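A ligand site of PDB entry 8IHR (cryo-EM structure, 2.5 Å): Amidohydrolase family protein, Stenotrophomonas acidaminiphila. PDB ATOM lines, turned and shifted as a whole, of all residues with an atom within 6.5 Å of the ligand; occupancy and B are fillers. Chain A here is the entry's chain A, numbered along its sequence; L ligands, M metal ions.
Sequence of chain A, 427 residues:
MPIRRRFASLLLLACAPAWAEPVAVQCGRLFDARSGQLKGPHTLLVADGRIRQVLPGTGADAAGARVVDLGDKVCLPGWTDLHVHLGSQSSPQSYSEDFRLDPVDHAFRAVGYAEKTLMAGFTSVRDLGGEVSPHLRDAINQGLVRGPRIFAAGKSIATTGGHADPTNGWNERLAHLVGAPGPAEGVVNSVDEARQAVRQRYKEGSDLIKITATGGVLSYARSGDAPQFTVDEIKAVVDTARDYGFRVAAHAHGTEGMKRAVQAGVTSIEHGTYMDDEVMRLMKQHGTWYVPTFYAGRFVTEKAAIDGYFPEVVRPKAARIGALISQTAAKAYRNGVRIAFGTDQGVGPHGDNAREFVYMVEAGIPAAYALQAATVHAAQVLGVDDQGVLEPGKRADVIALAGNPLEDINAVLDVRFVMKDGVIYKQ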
ATOM      1  N   HIS A  83       8.376   5.529 -20.636  1.00  0.00           N
ATOM      2  CA  HIS A  83       9.752   5.862 -20.272  1.00  0.00           C
ATOM      3  C   HIS A  83       9.870   7.382 -20.203  1.00  0.00           C
ATOM      4  O   HIS A  83       9.988   8.050 -21.236  1.00  0.00           O
ATOM      5  CB  HIS A  83      10.742   5.274 -21.270  1.00  0.00           C
ATOM      6  CG  HIS A  83      12.141   5.163 -20.752  1.00  0.00           C
ATOM      7  ND1 HIS A  83      13.014   4.181 -21.163  1.00  0.00           N
ATOM      8  CD2 HIS A  83      12.820   5.924 -19.860  1.00  0.00           C
ATOM      9  CE1 HIS A  83      14.174   4.334 -20.543  1.00  0.00           C
ATOM     10  NE2 HIS A  83      14.078   5.379 -19.747  1.00  0.00           N
ATOM     11  N   HIS A  85      11.560  10.676 -17.407  1.00  0.00           N
ATOM     12  CA  HIS A  85      12.289  11.104 -16.201  1.00  0.00           C
ATOM     13  C   HIS A  85      11.804  12.512 -15.896  1.00  0.00           C
ATOM     14  O   HIS A  85      12.414  13.494 -16.327  1.00  0.00           O
ATOM     15  CB  HIS A  85      13.805  11.054 -16.415  1.00  0.00           C
ATOM     16  CG  HIS A  85      14.330   9.697 -16.750  1.00  0.00           C
ATOM     17  ND1 HIS A  85      14.564   8.732 -15.792  1.00  0.00           N
ATOM     18  CD2 HIS A  85      14.667   9.134 -17.934  1.00  0.00           C
ATOM     19  CE1 HIS A  85      15.019   7.635 -16.371  1.00  0.00           C
ATOM     20  NE2 HIS A  85      15.095   7.852 -17.669  1.00  0.00           N
ATOM     21  N   HIS A 163      25.831   1.903 -14.831  1.00  0.00           N
ATOM     22  CA  HIS A 163      25.233   3.062 -15.490  1.00  0.00           C
ATOM     23  C   HIS A 163      24.443   3.925 -14.514  1.00  0.00           C
ATOM     24  O   HIS A 163      24.403   5.151 -14.664  1.00  0.00           O
ATOM     25  CB  HIS A 163      24.344   2.592 -16.640  1.00  0.00           C
ATOM     26  CG  HIS A 163      23.585   3.688 -17.317  1.00  0.00           C
ATOM     27  ND1 HIS A 163      24.207   4.719 -18.001  1.00  0.00           N
ATOM     28  CD2 HIS A 163      22.256   3.918 -17.418  1.00  0.00           C
ATOM     29  CE1 HIS A 163      23.295   5.530 -18.485  1.00  0.00           C
ATOM     30  NE2 HIS A 163      22.100   5.075 -18.147  1.00  0.00           N
ATOM     31  N   KCX A 210      13.520  -0.870 -11.512  1.00  0.00           N
ATOM     32  CA  KCX A 210      14.343  -0.548 -12.672  1.00  0.00           C
ATOM     33  CB  KCX A 210      14.263   0.947 -12.979  1.00  0.00           C
ATOM     34  CG  KCX A 210      14.215   1.305 -14.461  1.00  0.00           C
ATOM     35  CD  KCX A 210      15.430   0.808 -15.209  1.00  0.00           C
ATOM     36  CE  KCX A 210      15.523   1.456 -16.576  1.00  0.00           C
ATOM     37  NZ  KCX A 210      15.786   2.909 -16.465  1.00  0.00           N
ATOM     38  C   KCX A 210      15.792  -0.946 -12.424  1.00  0.00           C
ATOM     39  O   KCX A 210      16.399  -0.542 -11.431  1.00  0.00           O
ATOM     40  CX  KCX A 210      16.360   3.561 -17.471  1.00  0.00           C
ATOM     41  OQ1 KCX A 210      16.573   4.779 -17.365  1.00  0.00           O
ATOM     42  OQ2 KCX A 210      16.676   2.960 -18.492  1.00  0.00           O
ATOM     43  N   GLY A 215      26.134  -1.063 -19.546  1.00  0.00           N
ATOM     44  CA  GLY A 215      26.529   0.323 -19.463  1.00  0.00           C
ATOM     45  C   GLY A 215      25.596   1.209 -20.268  1.00  0.00           C
ATOM     46  O   GLY A 215      24.673   0.751 -20.948  1.00  0.00           O
ATOM     47  N   GLY A 216      25.846   2.514 -20.195  1.00  0.00           N
ATOM     48  CA  GLY A 216      24.993   3.481 -20.846  1.00  0.00           C
ATOM     49  C   GLY A 216      25.792   4.567 -21.550  1.00  0.00           C
ATOM     50  O   GLY A 216      27.020   4.537 -21.575  1.00  0.00           O
ATOM     51  N   VAL A 217      25.060   5.515 -22.110  1.00  0.00           N
ATOM     52  CA  VAL A 217      25.657   6.617 -22.867  1.00  0.00           C
ATOM     53  C   VAL A 217      25.934   7.816 -21.971  1.00  0.00           C
ATOM     54  O   VAL A 217      27.038   8.358 -21.955  1.00  0.00           O
ATOM     55  CB  VAL A 217      24.744   7.001 -24.045  1.00  0.00           C
ATOM     56  CG1 VAL A 217      25.152   8.332 -24.620  1.00  0.00           C
ATOM     57  CG2 VAL A 217      24.768   5.917 -25.114  1.00  0.00           C
ATOM     58  N   LEU A 218      24.932   8.253 -21.199  1.00  0.00           N
ATOM     59  CA  LEU A 218      25.040   9.493 -20.446  1.00  0.00           C
ATOM     60  C   LEU A 218      25.765   9.315 -19.110  1.00  0.00           C
ATOM     61  O   LEU A 218      25.975  10.309 -18.419  1.00  0.00           O
ATOM     62  CB  LEU A 218      23.652  10.084 -20.220  1.00  0.00           C
ATOM     63  CG  LEU A 218      22.877  10.461 -21.483  1.00  0.00           C
ATOM     64  CD1 LEU A 218      21.449  10.853 -21.148  1.00  0.00           C
ATOM     65  CD2 LEU A 218      23.570  11.570 -22.246  1.00  0.00           C
ATOM     66  N   SER A 219      26.138   8.098 -18.746  1.00  0.00           N
ATOM     67  CA  SER A 219      26.864   7.885 -17.505  1.00  0.00           C
ATOM     68  C   SER A 219      28.300   8.369 -17.635  1.00  0.00           C
ATOM     69  O   SER A 219      28.866   8.448 -18.728  1.00  0.00           O
ATOM     70  CB  SER A 219      26.827   6.408 -17.094  1.00  0.00           C
ATOM     71  OG  SER A 219      27.430   5.597 -18.086  1.00  0.00           O
ATOM     72  N   GLY A 224      30.004   1.465 -22.535  1.00  0.00           N
ATOM     73  CA  GLY A 224      28.670   1.814 -22.966  1.00  0.00           C
ATOM     74  C   GLY A 224      27.740   0.630 -23.135  1.00  0.00           C
ATOM     75  O   GLY A 224      26.515   0.818 -23.161  1.00  0.00           O
ATOM     76  N   HIS A 251      17.442  -1.785 -18.496  1.00  0.00           N
ATOM     77  CA  HIS A 251      18.170  -0.976 -19.467  1.00  0.00           C
ATOM     78  C   HIS A 251      19.333  -1.809 -20.000  1.00  0.00           C
ATOM     79  O   HIS A 251      20.155  -2.309 -19.213  1.00  0.00           O
ATOM     80  CB  HIS A 251      18.653   0.317 -18.806  1.00  0.00           C
ATOM     81  CG  HIS A 251      19.854   0.933 -19.470  1.00  0.00           C
ATOM     82  ND1 HIS A 251      19.768   2.075 -20.241  1.00  0.00           N
ATOM     83  CD2 HIS A 251      21.164   0.596 -19.442  1.00  0.00           C
ATOM     84  CE1 HIS A 251      20.974   2.397 -20.682  1.00  0.00           C
ATOM     85  NE2 HIS A 251      21.837   1.512 -20.214  1.00  0.00           N
ATOM     86  N   HIS A 253      22.072  -2.186 -23.583  1.00  0.00           N
ATOM     87  CA  HIS A 253      22.587  -1.868 -24.905  1.00  0.00           C
ATOM     88  C   HIS A 253      23.294  -3.051 -25.544  1.00  0.00           C
ATOM     89  O   HIS A 253      23.003  -3.388 -26.705  1.00  0.00           O
ATOM     90  CB  HIS A 253      23.563  -0.673 -24.827  1.00  0.00           C
ATOM     91  CG  HIS A 253      22.883   0.654 -24.682  1.00  0.00           C
ATOM     92  ND1 HIS A 253      21.898   1.082 -25.541  1.00  0.00           N
ATOM     93  CD2 HIS A 253      23.067   1.649 -23.790  1.00  0.00           C
ATOM     94  CE1 HIS A 253      21.494   2.291 -25.174  1.00  0.00           C
ATOM     95  NE2 HIS A 253      22.188   2.661 -24.118  1.00  0.00           N
ATOM     96  N   HIS A 271      15.824   0.260 -24.928  1.00  0.00           N
ATOM     97  CA  HIS A 271      16.728   0.749 -25.975  1.00  0.00           C
ATOM     98  C   HIS A 271      17.291  -0.337 -26.887  1.00  0.00           C
ATOM     99  O   HIS A 271      17.715  -0.021 -28.003  1.00  0.00           O
ATOM    100  CB  HIS A 271      17.915   1.516 -25.391  1.00  0.00           C
ATOM    101  CG  HIS A 271      17.563   2.428 -24.256  1.00  0.00           C
ATOM    102  ND1 HIS A 271      16.843   3.582 -24.422  1.00  0.00           N
ATOM    103  CD2 HIS A 271      17.867   2.366 -22.936  1.00  0.00           C
ATOM    104  CE1 HIS A 271      16.694   4.187 -23.258  1.00  0.00           C
ATOM    105  NE2 HIS A 271      17.310   3.473 -22.338  1.00  0.00           N
ATOM    106  N   THR A 273      19.710  -1.864 -28.122  1.00  0.00           N
ATOM    107  CA  THR A 273      20.513  -1.293 -29.211  1.00  0.00           C
ATOM    108  C   THR A 273      21.179  -2.367 -30.068  1.00  0.00           C
ATOM    109  O   THR A 273      21.082  -2.326 -31.303  1.00  0.00           O
ATOM    110  CB  THR A 273      21.559  -0.333 -28.651  1.00  0.00           C
ATOM    111  OG1 THR A 273      20.936   0.554 -27.719  1.00  0.00           O
ATOM    112  CG2 THR A 273      22.177   0.482 -29.762  1.00  0.00           C
ATOM    113  N   PRO A 292      11.813   0.944 -27.798  1.00  0.00           N
ATOM    114  CA  PRO A 292      12.977   1.429 -28.551  1.00  0.00           C
ATOM    115  C   PRO A 292      13.481   2.802 -28.144  1.00  0.00           C
ATOM    116  O   PRO A 292      14.696   2.993 -28.015  1.00  0.00           O
ATOM    117  CB  PRO A 292      12.469   1.431 -30.003  1.00  0.00           C
ATOM    118  CG  PRO A 292      11.245   0.576 -29.995  1.00  0.00           C
ATOM    119  CD  PRO A 292      10.631   0.747 -28.654  1.00  0.00           C
ATOM    120  N   THR A 293      12.585   3.776 -27.924  1.00  0.00           N
ATOM    121  CA  THR A 293      12.927   5.163 -27.603  1.00  0.00           C
ATOM    122  C   THR A 293      13.756   5.811 -28.724  1.00  0.00           C
ATOM    123  O   THR A 293      14.950   6.091 -28.586  1.00  0.00           O
ATOM    124  CB  THR A 293      13.659   5.267 -26.253  1.00  0.00           C
ATOM    125  OG1 THR A 293      15.010   4.826 -26.403  1.00  0.00           O
ATOM    126  CG2 THR A 293      12.966   4.441 -25.186  1.00  0.00           C
ATOM    127  N   ALA A 296      15.264   9.588 -27.823  1.00  0.00           N
ATOM    128  CA  ALA A 296      16.512   9.738 -27.088  1.00  0.00           C
ATOM    129  C   ALA A 296      17.712   9.493 -27.988  1.00  0.00           C
ATOM    130  O   ALA A 296      18.724  10.206 -27.895  1.00  0.00           O
ATOM    131  CB  ALA A 296      16.537   8.792 -25.893  1.00  0.00           C
ATOM    132  N   GLY A 297      17.628   8.492 -28.858  1.00  0.00           N
ATOM    133  CA  GLY A 297      18.713   8.238 -29.792  1.00  0.00           C
ATOM    134  C   GLY A 297      18.960   9.415 -30.721  1.00  0.00           C
ATOM    135  O   GLY A 297      20.111   9.836 -30.920  1.00  0.00           O
ATOM    136  N   ARG A 298      17.892   9.963 -31.299  1.00  0.00           N
ATOM    137  CA  ARG A 298      18.057  11.127 -32.169  1.00  0.00           C
ATOM    138  C   ARG A 298      18.624  12.315 -31.409  1.00  0.00           C
ATOM    139  O   ARG A 298      19.493  13.034 -31.926  1.00  0.00           O
ATOM    140  CB  ARG A 298      16.725  11.493 -32.828  1.00  0.00           C
ATOM    141  CG  ARG A 298      16.338  10.588 -33.981  1.00  0.00           C
ATOM    142  CD  ARG A 298      15.044  11.039 -34.624  1.00  0.00           C
ATOM    143  NE  ARG A 298      15.274  11.802 -35.834  1.00  0.00           N
ATOM    144  CZ  ARG A 298      14.779  11.494 -37.028  1.00  0.00           C
ATOM    145  NH1 ARG A 298      14.009  10.427 -37.198  1.00  0.00           N
ATOM    146  NH2 ARG A 298      15.054  12.261 -38.071  1.00  0.00           N
ATOM    147  N   VAL A 300      20.557  12.364 -28.642  1.00  0.00           N
ATOM    148  CA  VAL A 300      21.958  12.206 -28.288  1.00  0.00           C
ATOM    149  C   VAL A 300      22.839  12.235 -29.538  1.00  0.00           C
ATOM    150  O   VAL A 300      23.989  12.671 -29.479  1.00  0.00           O
ATOM    151  CB  VAL A 300      22.200  10.930 -27.455  1.00  0.00           C
ATOM    152  CG1 VAL A 300      21.418  10.993 -26.153  1.00  0.00           C
ATOM    153  CG2 VAL A 300      21.854   9.683 -28.245  1.00  0.00           C
ATOM    154  N   LYS A 317      30.587   7.746 -26.936  1.00  0.00           N
ATOM    155  CA  LYS A 317      29.535   6.760 -26.737  1.00  0.00           C
ATOM    156  C   LYS A 317      28.218   7.228 -27.335  1.00  0.00           C
ATOM    157  O   LYS A 317      27.504   6.445 -27.973  1.00  0.00           O
ATOM    158  CB  LYS A 317      29.364   6.470 -25.246  1.00  0.00           C
ATOM    159  CG  LYS A 317      30.626   5.981 -24.557  1.00  0.00           C
ATOM    160  CD  LYS A 317      30.350   5.586 -23.110  1.00  0.00           C
ATOM    161  CE  LYS A 317      29.959   6.785 -22.270  1.00  0.00           C
ATOM    162  NZ  LYS A 317      29.534   6.408 -20.901  1.00  0.00           N
ATOM    163  N   ALA A 318      27.881   8.508 -27.148  1.00  0.00           N
ATOM    164  CA  ALA A 318      26.663   9.055 -27.739  1.00  0.00           C
ATOM    165  C   ALA A 318      26.706   8.942 -29.252  1.00  0.00           C
ATOM    166  O   ALA A 318      25.764   8.443 -29.883  1.00  0.00           O
ATOM    167  CB  ALA A 318      26.478  10.508 -27.309  1.00  0.00           C
ATOM    168  N   ILE A 321      26.390   5.153 -30.324  1.00  0.00           N
ATOM    169  CA  ILE A 321      25.207   4.362 -29.989  1.00  0.00           C
ATOM    170  C   ILE A 321      23.908   5.004 -30.463  1.00  0.00           C
ATOM    171  O   ILE A 321      22.940   4.281 -30.745  1.00  0.00           O
ATOM    172  CB  ILE A 321      25.192   4.109 -28.468  1.00  0.00           C
ATOM    173  CG1 ILE A 321      26.440   3.332 -28.044  1.00  0.00           C
ATOM    174  CG2 ILE A 321      23.944   3.329 -28.059  1.00  0.00           C
ATOM    175  CD1 ILE A 321      26.423   2.864 -26.614  1.00  0.00           C
ATOM    176  N   GLY A 322      23.844   6.332 -30.584  1.00  0.00           N
ATOM    177  CA  GLY A 322      22.593   6.974 -30.932  1.00  0.00           C
ATOM    178  C   GLY A 322      22.065   6.573 -32.297  1.00  0.00           C
ATOM    179  O   GLY A 322      20.858   6.436 -32.499  1.00  0.00           O
ATOM    180  N   ILE A 325      19.332   2.951 -33.156  1.00  0.00           N
ATOM    181  CA  ILE A 325      17.990   2.592 -32.606  1.00  0.00           C
ATOM    182  C   ILE A 325      16.992   2.364 -33.731  1.00  0.00           C
ATOM    183  O   ILE A 325      16.254   1.372 -33.665  1.00  0.00           O
ATOM    184  CB  ILE A 325      17.520   3.680 -31.614  1.00  0.00           C
ATOM    185  CG1 ILE A 325      18.546   3.917 -30.497  1.00  0.00           C
ATOM    186  CG2 ILE A 325      16.140   3.364 -31.071  1.00  0.00           C
ATOM    187  CD1 ILE A 325      18.537   2.845 -29.429  1.00  0.00           C
ATOM    188  N   ASP A 344      11.662   8.213 -23.375  1.00  0.00           N
ATOM    189  CA  ASP A 344      12.823   8.615 -22.520  1.00  0.00           C
ATOM    190  C   ASP A 344      12.910  10.151 -22.376  1.00  0.00           C
ATOM    191  O   ASP A 344      14.031  10.662 -22.349  1.00  0.00           O
ATOM    192  CB  ASP A 344      14.137   7.997 -22.998  1.00  0.00           C
ATOM    193  CG  ASP A 344      15.237   7.955 -21.959  1.00  0.00           C
ATOM    194  OD1 ASP A 344      15.010   8.455 -20.851  1.00  0.00           O
ATOM    195  OD2 ASP A 344      16.308   7.404 -22.267  1.00  0.00           O
ATOM    196  N   VAL A 347      15.771  13.347 -21.468  1.00  0.00           N
ATOM    197  CA  VAL A 347      16.941  13.588 -22.346  1.00  0.00           C
ATOM    198  C   VAL A 347      16.377  14.617 -23.317  1.00  0.00           C
ATOM    199  O   VAL A 347      16.995  15.682 -23.446  1.00  0.00           O
ATOM    200  CB  VAL A 347      17.405  12.295 -23.062  1.00  0.00           C
ATOM    201  CG1 VAL A 347      18.578  12.563 -24.002  1.00  0.00           C
ATOM    202  CG2 VAL A 347      17.752  11.191 -22.088  1.00  0.00           C
HETATM  203  N1  LIG L   1      19.364   6.940 -21.243  1.00  0.00           N
HETATM  204  C1  LIG L   1      20.120   6.436 -22.378  1.00  0.00           C
HETATM  205  C2  LIG L   1      21.580   6.221 -21.997  1.00  0.00           C
HETATM  206  O1  LIG L   1      22.197   7.072 -21.347  1.00  0.00           O
HETATM  207  C3  LIG L   1      20.024   7.411 -23.559  1.00  0.00           C
HETATM  208  C4  LIG L   1      20.014   6.749 -24.900  1.00  0.00           C
HETATM  209  C5  LIG L   1      18.905   6.046 -25.338  1.00  0.00           C
HETATM  210  C6  LIG L   1      21.124   6.822 -25.730  1.00  0.00           C
HETATM  211  C7  LIG L   1      18.898   5.436 -26.577  1.00  0.00           C
HETATM  212  C8  LIG L   1      21.121   6.208 -26.961  1.00  0.00           C
HETATM  213  C9  LIG L   1      20.006   5.522 -27.387  1.00  0.00           C
HETATM  214  O2  LIG L   1      22.176   5.202 -22.317  1.00  0.00           O
HETATM  215 ZN    ZN M   1      18.160   3.721 -20.209  1.00  0.00          ZN
HETATM  216 ZN    ZN M   2      16.066   6.347 -19.112  1.00  0.00          ZN
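His 163 touches the ligand. Gly 216 touches the ligand (CA to O2, 3.6 Å). His 251 touches the ligand (CE1 to O2, 3.5 Å). His 271 touches the ligand. OG1 of Thr 293 touches C7 of the ligand, at 3.9 Å. Ala 296 touches the ligand. Gly 297 touches the ligand. Val 300 touches the ligand. Ile 325 touches the ligand (CD1 to C9, 3.7 Å). Hydrophobic or aromatic side chains within 4 Å of the ligand: His 163, Val 217, Leu 218, His 251, His 253, His 271, Ala 296, Val 300 and Ile 325. Within 4 Å of the ligand: His 163, Gly 216, Val 217, Leu 218, His 251, His 253, His 271, Thr 293, Ala 296, Gly 297, Val 300, Ile 325 and Asp 344.
The backbone NH of Val 217 lies within hydrogen-bond range of an oxygen (O2) of the ligand, at 2.9 Å. N of Leu 218 is in hydrogen-bond range of O1 of the ligand, 3.0 Å away. An oxygen (O2) of the ligand is in hydrogen-bond range of a ring nitrogen (NE2) of His 253, at 3.1 Å. OD2 of Asp 344 is in salt-bridge range of N1 of the ligand.
NZ of Lys 317 sits close to O of Val 217 (3.3 Å). NE2 of His 85 lies close to OD1 of Asp 344 (3.2 Å). The side-chain hydroxyl of Thr 293 sits at hydrogen-bond distance from a ring nitrogen (ND1) of His 271 (3.0 Å). The side-chain hydroxyl (OG1) of Thr 273 sits at hydrogen-bond distance from the backbone carbonyl oxygen (O) of His 271. ND1 of His 163 sits close to OG of Ser 219 (3.3 Å). The backbone carbonyl oxygen (O) of Gly 215 sits at hydrogen-bond distance from a ring nitrogen (NE2) of His 251 (3.0 Å). The backbone carbonyl oxygen of Gly 224 sits at hydrogen-bond distance from the backbone NH of Gly 216 (3.5 Å). NZ of Lys 317 sits at hydrogen-bond distance from O of Gly 216.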
